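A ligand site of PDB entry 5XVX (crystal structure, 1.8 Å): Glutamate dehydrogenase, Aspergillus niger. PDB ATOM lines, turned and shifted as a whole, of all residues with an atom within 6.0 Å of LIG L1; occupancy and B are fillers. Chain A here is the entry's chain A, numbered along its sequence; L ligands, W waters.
OG1 of Thr 181 is in hydrogen-bond range of NZ of Lys 78, at 2.9 Å. N of Gly 382 sits close to OG1 of Thr 197 (3.5 Å). The side-chain hydroxyl (OG) of Ser 386 sits at hydrogen-bond distance from the side-chain hydroxyl (OG1) of Thr 181. The side-chain amino group (NZ) of Lys 78 lies within hydrogen-bond range of the backbone carbonyl oxygen (O) of Val 150, 2.9 Å away. OD1 of Asn 346 is in hydrogen-bond range of ND2 of Asn 379 (3.2 Å). OD1 of Asn 103 sits close to O of Gln 99. The side-chain amino group (NZ) of Lys 102 is in hydrogen-bond range of the side-chain amide oxygen (OE1) of Gln 99 (3.5 Å). The side-chain amide nitrogen (ND2) of Asn 103 is in hydrogen-bond range of the backbone carbonyl oxygen (O) of Lys 78 (3.3 Å).
An oxygen (O2) of LIG L1 is in hydrogen-bond range of the side-chain amide nitrogen (ND2) of Asn 346. An oxygen (O14) of LG2 L2 is in hydrogen-bond range of the guanidinium group of Arg 193 (2.9 Å). The guanidinium group (NH2) of Arg 193 lies within salt-bridge range of an oxygen (O4) of LIG L1. An oxygen (O5) of LIG L1 is in salt-bridge range of the side-chain amino group (NZ) of Lys 78, 2.7 Å away. The backbone NH (N) of Asn 346 sits at hydrogen-bond distance from an oxygen (O12) of LG2 L2 (3.0 Å). An oxygen (O14) of LG2 L2 lies within hydrogen-bond range of the side-chain hydroxyl of Thr 197, 2.6 Å away. NE2 of Gln 99 is in hydrogen-bond range of O1 of LIG L1, at 2.9 Å. ND2 of Asn 346 lies within hydrogen-bond range of O13 of LG2 L2. NZ of Lys 114 is in salt-bridge range of O2 of LIG L1 (2.9 Å). The side-chain hydroxyl (OG) of Ser 386 sits at hydrogen-bond distance from an oxygen (O4) of LIG L1. OD1 of Asp 154 sits at hydrogen-bond distance from O13 of LG2 L2. The side-chain amino group (NZ) of Lys 102 lies within salt-bridge range of an oxygen (O1) of LIG L1 (2.7 Å).
The backbone carbonyl oxygen (O) of Gly 153 lies close to an oxygen (O3) of LIG L1 (3.4 Å). The side-chain carboxylate (OD1) of Asp 154 lies close to an oxygen (O3) of LIG L1, 2.9 Å away. Residues that only touch LIG L1: Gly 79, Gly 80, Ala 152, Gly 382 and Val 383. The nearest printed residue that does not touch LIG L1 is Thr 181 (4.1 Å).
Water W1 lies within hydrogen-bond range of O of Asn 379 (2.7 Å), N of Val 383 (2.8 Å), O1 of LIG L1 (2.8 Å) and N of Gly 382 (3.4 Å).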
ATOM      1  N   LYS A  78      36.737 -18.802   3.851  1.00  0.00           N
ATOM      2  CA  LYS A  78      36.412 -17.987   4.979  1.00  0.00           C
ATOM      3  C   LYS A  78      35.135 -18.557   5.598  1.00  0.00           C
ATOM      4  O   LYS A  78      34.164 -18.844   4.881  1.00  0.00           O
ATOM      5  CB  LYS A  78      36.119 -16.567   4.563  1.00  0.00           C
ATOM      6  CG  LYS A  78      35.874 -15.621   5.724  1.00  0.00           C
ATOM      7  CD  LYS A  78      37.179 -15.151   6.301  1.00  0.00           C
ATOM      8  CE  LYS A  78      37.026 -14.450   7.644  1.00  0.00           C
ATOM      9  NZ  LYS A  78      36.834 -15.365   8.816  1.00  0.00           N
ATOM     10  N   GLY A  79      35.189 -18.774   6.898  1.00  0.00           N
ATOM     11  CA  GLY A  79      34.000 -19.171   7.655  1.00  0.00           C
ATOM     12  C   GLY A  79      34.414 -19.754   8.982  1.00  0.00           C
ATOM     13  O   GLY A  79      35.575 -20.074   9.218  1.00  0.00           O
ATOM     14  N   GLY A  80      33.463 -19.909   9.869  1.00  0.00           N
ATOM     15  CA  GLY A  80      33.746 -20.281  11.235  1.00  0.00           C
ATOM     16  C   GLY A  80      34.038 -21.719  11.570  1.00  0.00           C
ATOM     17  O   GLY A  80      34.004 -22.603  10.713  1.00  0.00           O
ATOM     18  N   LEU A  95      26.906 -25.786   6.065  1.00  0.00           N
ATOM     19  CA  LEU A  95      27.395 -24.481   6.510  1.00  0.00           C
ATOM     20  C   LEU A  95      28.381 -23.861   5.526  1.00  0.00           C
ATOM     21  O   LEU A  95      28.285 -22.659   5.179  1.00  0.00           O
ATOM     22  CB  LEU A  95      27.990 -24.588   7.887  1.00  0.00           C
ATOM     23  CG  LEU A  95      26.987 -24.796   9.034  1.00  0.00           C
ATOM     24  CD1 LEU A  95      27.654 -25.422  10.243  1.00  0.00           C
ATOM     25  CD2 LEU A  95      26.311 -23.475   9.371  1.00  0.00           C
ATOM     26  N   GLN A  99      27.964 -20.584   3.146  1.00  0.00           N
ATOM     27  CA  GLN A  99      29.005 -19.583   3.311  1.00  0.00           C
ATOM     28  C   GLN A  99      29.526 -19.018   1.985  1.00  0.00           C
ATOM     29  O   GLN A  99      29.888 -17.817   1.915  1.00  0.00           O
ATOM     30  CB  GLN A  99      30.182 -20.145   4.151  1.00  0.00           C
ATOM     31  CG  GLN A  99      30.954 -19.070   4.881  1.00  0.00           C
ATOM     32  CD  GLN A  99      30.234 -18.534   6.094  1.00  0.00           C
ATOM     33  OE1 GLN A  99      29.399 -19.209   6.659  1.00  0.00           O
ATOM     34  NE2 GLN A  99      30.571 -17.330   6.508  1.00  0.00           N
ATOM     35  N   LYS A 102      26.754 -16.441   0.905  1.00  0.00           N
ATOM     36  CA  LYS A 102      26.757 -15.389   1.907  1.00  0.00           C
ATOM     37  C   LYS A 102      27.949 -14.468   1.686  1.00  0.00           C
ATOM     38  O   LYS A 102      27.835 -13.225   1.636  1.00  0.00           O
ATOM     39  CB  LYS A 102      26.838 -16.004   3.291  1.00  0.00           C
ATOM     40  CG  LYS A 102      26.825 -14.992   4.451  1.00  0.00           C
ATOM     41  CD  LYS A 102      27.144 -15.615   5.791  1.00  0.00           C
ATOM     42  CE  LYS A 102      26.413 -16.919   6.063  1.00  0.00           C
ATOM     43  NZ  LYS A 102      26.554 -17.346   7.477  1.00  0.00           N
ATOM     44  N   ASN A 103      29.123 -15.087   1.543  1.00  0.00           N
ATOM     45  CA  ASN A 103      30.329 -14.275   1.383  1.00  0.00           C
ATOM     46  C   ASN A 103      30.284 -13.446   0.122  1.00  0.00           C
ATOM     47  O   ASN A 103      30.726 -12.297   0.112  1.00  0.00           O
ATOM     48  CB  ASN A 103      31.603 -15.152   1.508  1.00  0.00           C
ATOM     49  CG  ASN A 103      31.756 -15.708   2.914  1.00  0.00           C
ATOM     50  OD1 ASN A 103      30.891 -15.501   3.812  1.00  0.00           O
ATOM     51  ND2 ASN A 103      32.837 -16.431   3.135  1.00  0.00           N
ATOM     52  N   LYS A 114      34.041 -23.894   6.209  1.00  0.00           N
ATOM     53  CA  LYS A 114      33.548 -24.063   7.586  1.00  0.00           C
ATOM     54  C   LYS A 114      34.285 -25.238   8.192  1.00  0.00           C
ATOM     55  O   LYS A 114      34.652 -26.178   7.455  1.00  0.00           O
ATOM     56  CB  LYS A 114      32.031 -24.394   7.566  1.00  0.00           C
ATOM     57  CG  LYS A 114      31.354 -23.964   8.843  1.00  0.00           C
ATOM     58  CD  LYS A 114      31.059 -22.478   8.829  1.00  0.00           C
ATOM     59  CE  LYS A 114      30.365 -22.046  10.104  1.00  0.00           C
ATOM     60  NZ  LYS A 114      29.935 -20.665   9.889  1.00  0.00           N
ATOM     61  N   VAL A 150      40.827 -18.557   6.411  1.00  0.00           N
ATOM     62  CA  VAL A 150      40.780 -17.724   7.596  1.00  0.00           C
ATOM     63  C   VAL A 150      39.532 -18.131   8.395  1.00  0.00           C
ATOM     64  O   VAL A 150      38.440 -17.679   8.076  1.00  0.00           O
ATOM     65  CB  VAL A 150      40.762 -16.231   7.236  1.00  0.00           C
ATOM     66  CG1 VAL A 150      40.688 -15.347   8.474  1.00  0.00           C
ATOM     67  CG2 VAL A 150      42.004 -15.851   6.461  1.00  0.00           C
ATOM     68  N   PRO A 151      39.703 -19.004   9.400  1.00  0.00           N
ATOM     69  CA  PRO A 151      38.569 -19.355  10.256  1.00  0.00           C
ATOM     70  C   PRO A 151      38.197 -18.252  11.270  1.00  0.00           C
ATOM     71  O   PRO A 151      38.727 -17.138  11.273  1.00  0.00           O
ATOM     72  CB  PRO A 151      38.998 -20.662  10.931  1.00  0.00           C
ATOM     73  CG  PRO A 151      40.148 -21.174  10.081  1.00  0.00           C
ATOM     74  CD  PRO A 151      40.841 -19.895   9.694  1.00  0.00           C
ATOM     75  N   ALA A 152      37.186 -18.568  12.058  1.00  0.00           N
ATOM     76  CA  ALA A 152      36.643 -17.655  13.043  1.00  0.00           C
ATOM     77  C   ALA A 152      35.796 -18.527  13.971  1.00  0.00           C
ATOM     78  O   ALA A 152      35.861 -19.756  13.902  1.00  0.00           O
ATOM     79  CB  ALA A 152      35.796 -16.602  12.374  1.00  0.00           C
ATOM     80  N   GLY A 153      35.007 -17.895  14.842  1.00  0.00           N
ATOM     81  CA  GLY A 153      34.077 -18.625  15.698  1.00  0.00           C
ATOM     82  C   GLY A 153      32.815 -19.064  14.971  1.00  0.00           C
ATOM     83  O   GLY A 153      32.674 -18.853  13.768  1.00  0.00           O
ATOM     84  N   ASP A 154      31.954 -19.751  15.719  1.00  0.00           N
ATOM     85  CA  ASP A 154      30.571 -20.093  15.341  1.00  0.00           C
ATOM     86  C   ASP A 154      30.072 -20.725  16.647  1.00  0.00           C
ATOM     87  O   ASP A 154      30.565 -20.371  17.724  1.00  0.00           O
ATOM     88  CB  ASP A 154      30.546 -21.091  14.178  1.00  0.00           C
ATOM     89  CG  ASP A 154      29.150 -21.255  13.547  1.00  0.00           C
ATOM     90  OD1 ASP A 154      28.698 -20.405  12.735  1.00  0.00           O
ATOM     91  OD2 ASP A 154      28.510 -22.309  13.846  1.00  0.00           O
ATOM     92  N   THR A 181      39.771 -14.668  12.455  1.00  0.00           N
ATOM     93  CA  THR A 181      39.099 -13.473  12.864  1.00  0.00           C
ATOM     94  C   THR A 181      38.275 -13.741  14.132  1.00  0.00           C
ATOM     95  O   THR A 181      38.201 -14.883  14.624  1.00  0.00           O
ATOM     96  CB  THR A 181      38.246 -12.881  11.715  1.00  0.00           C
ATOM     97  OG1 THR A 181      37.286 -13.857  11.289  1.00  0.00           O
ATOM     98  CG2 THR A 181      39.151 -12.453  10.569  1.00  0.00           C
ATOM     99  N   ARG A 193      33.401  -6.361  15.732  1.00  0.00           N
ATOM    100  CA  ARG A 193      33.223  -7.782  15.411  1.00  0.00           C
ATOM    101  C   ARG A 193      32.325  -8.570  16.385  1.00  0.00           C
ATOM    102  O   ARG A 193      31.523  -9.406  15.938  1.00  0.00           O
ATOM    103  CB  ARG A 193      34.574  -8.530  15.187  1.00  0.00           C
ATOM    104  CG  ARG A 193      34.395  -9.991  14.768  1.00  0.00           C
ATOM    105  CD  ARG A 193      33.747 -10.092  13.388  1.00  0.00           C
ATOM    106  NE  ARG A 193      33.353 -11.451  12.969  1.00  0.00           N
ATOM    107  CZ  ARG A 193      32.215 -12.068  13.312  1.00  0.00           C
ATOM    108  NH1 ARG A 193      31.338 -11.502  14.150  1.00  0.00           N
ATOM    109  NH2 ARG A 193      31.937 -13.259  12.805  1.00  0.00           N
ATOM    110  N   THR A 197      27.266  -9.674  13.829  1.00  0.00           N
ATOM    111  CA  THR A 197      26.263 -10.539  13.240  1.00  0.00           C
ATOM    112  C   THR A 197      24.845 -10.076  13.665  1.00  0.00           C
ATOM    113  O   THR A 197      23.965  -9.855  12.827  1.00  0.00           O
ATOM    114  CB  THR A 197      26.494 -12.009  13.564  1.00  0.00           C
ATOM    115  OG1 THR A 197      27.834 -12.352  13.094  1.00  0.00           O
ATOM    116  CG2 THR A 197      25.507 -12.868  12.826  1.00  0.00           C
ATOM    117  N   ASN A 346      22.265 -19.961  10.841  1.00  0.00           N
ATOM    118  CA  ASN A 346      22.354 -20.551   9.532  1.00  0.00           C
ATOM    119  C   ASN A 346      21.302 -21.670   9.359  1.00  0.00           C
ATOM    120  O   ASN A 346      21.191 -22.566  10.162  1.00  0.00           O
ATOM    121  CB  ASN A 346      23.782 -21.100   9.299  1.00  0.00           C
ATOM    122  CG  ASN A 346      24.759 -19.964   9.086  1.00  0.00           C
ATOM    123  OD1 ASN A 346      24.593 -19.172   8.150  1.00  0.00           O
ATOM    124  ND2 ASN A 346      25.766 -19.859   9.942  1.00  0.00           N
ATOM    125  N   ASN A 379      22.428 -12.565   8.015  1.00  0.00           N
ATOM    126  CA  ASN A 379      23.451 -12.811   9.025  1.00  0.00           C
ATOM    127  C   ASN A 379      24.887 -12.580   8.485  1.00  0.00           C
ATOM    128  O   ASN A 379      25.833 -12.771   9.234  1.00  0.00           O
ATOM    129  CB  ASN A 379      23.289 -14.168   9.724  1.00  0.00           C
ATOM    130  CG  ASN A 379      23.746 -15.363   8.903  1.00  0.00           C
ATOM    131  OD1 ASN A 379      24.699 -15.281   8.122  1.00  0.00           O
ATOM    132  ND2 ASN A 379      23.104 -16.503   9.105  1.00  0.00           N
ATOM    133  N   ALA A 380      24.979 -12.054   7.282  1.00  0.00           N
ATOM    134  CA  ALA A 380      26.259 -11.795   6.591  1.00  0.00           C
ATOM    135  C   ALA A 380      27.097 -10.702   7.224  1.00  0.00           C
ATOM    136  O   ALA A 380      28.247 -10.528   6.829  1.00  0.00           O
ATOM    137  CB  ALA A 380      25.999 -11.406   5.144  1.00  0.00           C
ATOM    138  N   GLY A 382      28.458 -10.643  10.132  1.00  0.00           N
ATOM    139  CA  GLY A 382      29.551 -11.201  10.926  1.00  0.00           C
ATOM    140  C   GLY A 382      30.751 -11.436  10.037  1.00  0.00           C
ATOM    141  O   GLY A 382      31.822 -10.900  10.293  1.00  0.00           O
ATOM    142  N   VAL A 383      30.529 -12.205   9.000  1.00  0.00           N
ATOM    143  CA  VAL A 383      31.611 -12.485   8.040  1.00  0.00           C
ATOM    144  C   VAL A 383      32.108 -11.200   7.336  1.00  0.00           C
ATOM    145  O   VAL A 383      33.299 -11.078   7.041  1.00  0.00           O
ATOM    146  CB  VAL A 383      31.252 -13.648   7.097  1.00  0.00           C
ATOM    147  CG1 VAL A 383      30.311 -13.230   5.996  1.00  0.00           C
ATOM    148  CG2 VAL A 383      32.566 -14.201   6.484  1.00  0.00           C
ATOM    149  N   ALA A 384      31.227 -10.243   7.039  1.00  0.00           N
ATOM    150  CA  ALA A 384      31.628  -8.983   6.492  1.00  0.00           C
ATOM    151  C   ALA A 384      32.592  -8.271   7.424  1.00  0.00           C
ATOM    152  O   ALA A 384      33.670  -7.825   6.961  1.00  0.00           O
ATOM    153  CB  ALA A 384      30.410  -8.089   6.190  1.00  0.00           C
ATOM    154  N   SER A 386      34.361  -9.718   9.769  1.00  0.00           N
ATOM    155  CA  SER A 386      35.592 -10.560   9.678  1.00  0.00           C
ATOM    156  C   SER A 386      36.470 -10.143   8.492  1.00  0.00           C
ATOM    157  O   SER A 386      37.688 -10.044   8.641  1.00  0.00           O
ATOM    158  CB  SER A 386      35.275 -12.055   9.582  1.00  0.00           C
ATOM    159  OG  SER A 386      34.949 -12.615  10.838  1.00  0.00           O
HETATM  160  C1  LIG L   1      28.919 -17.301   9.772  1.00  0.00           C
HETATM  161  O1  LIG L   1      28.837 -16.550   8.756  1.00  0.00           O
HETATM  162  O2  LIG L   1      28.205 -18.298   9.782  1.00  0.00           O
HETATM  163  C2  LIG L   1      29.864 -17.097  10.913  1.00  0.00           C
HETATM  164  O3  LIG L   1      29.946 -17.893  11.917  1.00  0.00           O
HETATM  165  C3  LIG L   1      30.842 -15.935  10.839  1.00  0.00           C
HETATM  166  C4  LIG L   1      32.068 -16.496  10.150  1.00  0.00           C
HETATM  167  C5  LIG L   1      33.255 -15.570   9.994  1.00  0.00           C
HETATM  168  O4  LIG L   1      33.296 -14.463  10.584  1.00  0.00           O
HETATM  169  O5  LIG L   1      34.206 -16.000   9.252  1.00  0.00           O
HETATM  170  P1  LG2 L   2      26.897 -19.381  20.318  1.00  0.00           P
HETATM  171  O1  LG2 L   2      27.427 -18.111  20.943  1.00  0.00           O
HETATM  172  O2  LG2 L   2      27.555 -20.684  20.655  1.00  0.00           O
HETATM  173  O3  LG2 L   2      25.362 -19.509  20.708  1.00  0.00           O
HETATM  174  C1  LG2 L   2      24.583 -20.566  20.187  1.00  0.00           C
HETATM  175  C2  LG2 L   2      23.139 -20.527  20.888  1.00  0.00           C
HETATM  176  O4  LG2 L   2      22.344 -21.395  20.273  1.00  0.00           O
HETATM  177  C3  LG2 L   2      23.201 -20.931  22.360  1.00  0.00           C
HETATM  178  O5  LG2 L   2      22.217 -20.215  23.140  1.00  0.00           O
HETATM  179  C4  LG2 L   2      22.937 -22.415  22.164  1.00  0.00           C
HETATM  180  O6  LG2 L   2      22.440 -22.976  23.436  1.00  0.00           O
HETATM  181  C5  LG2 L   2      22.006 -22.554  21.205  1.00  0.00           C
HETATM  182  N1  LG2 L   2      22.172 -23.771  20.497  1.00  0.00           N
HETATM  183  C6  LG2 L   2      23.280 -24.271  19.844  1.00  0.00           C
HETATM  184  N2  LG2 L   2      23.019 -25.499  19.350  1.00  0.00           N
HETATM  185  C7  LG2 L   2      21.732 -25.741  19.670  1.00  0.00           C
HETATM  186  C8  LG2 L   2      21.004 -26.887  19.387  1.00  0.00           C
HETATM  187  N3  LG2 L   2      21.399 -28.063  18.676  1.00  0.00           N
HETATM  188  N4  LG2 L   2      19.728 -26.981  19.805  1.00  0.00           N
HETATM  189  C9  LG2 L   2      19.171 -25.923  20.498  1.00  0.00           C
HETATM  190  N5  LG2 L   2      19.880 -24.766  20.815  1.00  0.00           N
HETATM  191  C10 LG2 L   2      21.193 -24.708  20.382  1.00  0.00           C
HETATM  192  O7  LG2 L   2      26.828 -19.270  18.739  1.00  0.00           O
HETATM  193  P2  LG2 L   2      26.473 -18.076  17.750  1.00  0.00           P
HETATM  194  O8  LG2 L   2      25.597 -17.074  18.498  1.00  0.00           O
HETATM  195  O9  LG2 L   2      27.743 -17.460  17.258  1.00  0.00           O
HETATM  196  O10 LG2 L   2      25.737 -18.790  16.594  1.00  0.00           O
HETATM  197  C11 LG2 L   2      24.276 -18.861  16.498  1.00  0.00           C
HETATM  198  C12 LG2 L   2      23.846 -19.037  15.056  1.00  0.00           C
HETATM  199  O11 LG2 L   2      24.256 -17.976  14.314  1.00  0.00           O
HETATM  200  C13 LG2 L   2      24.379 -20.335  14.375  1.00  0.00           C
HETATM  201  O12 LG2 L   2      23.480 -20.868  13.472  1.00  0.00           O
HETATM  202  C14 LG2 L   2      25.618 -19.712  13.679  1.00  0.00           C
HETATM  203  O13 LG2 L   2      26.102 -20.630  12.636  1.00  0.00           O
HETATM  204  C15 LG2 L   2      25.124 -18.561  13.142  1.00  0.00           C
HETATM  205  N6  LG2 L   2      25.989 -17.487  12.786  1.00  0.00           N
HETATM  206  C16 LG2 L   2      27.022 -17.116  13.585  1.00  0.00           C
HETATM  207  C17 LG2 L   2      27.974 -16.105  13.153  1.00  0.00           C
HETATM  208  C18 LG2 L   2      28.839 -15.346  14.136  1.00  0.00           C
HETATM  209  O14 LG2 L   2      29.416 -14.342  13.745  1.00  0.00           O
HETATM  210  N7  LG2 L   2      28.943 -15.754  15.483  1.00  0.00           N
HETATM  211  C19 LG2 L   2      27.777 -15.385  11.839  1.00  0.00           C
HETATM  212  C20 LG2 L   2      26.646 -15.862  10.988  1.00  0.00           C
HETATM  213  C21 LG2 L   2      25.638 -16.755  11.621  1.00  0.00           C
HETATM  214  P3  LG2 L   2      23.331 -23.998  24.351  1.00  0.00           P
HETATM  215  O15 LG2 L   2      22.368 -24.554  25.425  1.00  0.00           O
HETATM  216  O16 LG2 L   2      24.411 -23.264  24.977  1.00  0.00           O
HETATM  217  O17 LG2 L   2      23.758 -25.156  23.416  1.00  0.00           O
HETATM  218  O   HOH W   1      28.258 -13.784   8.855  1.00  0.00           O
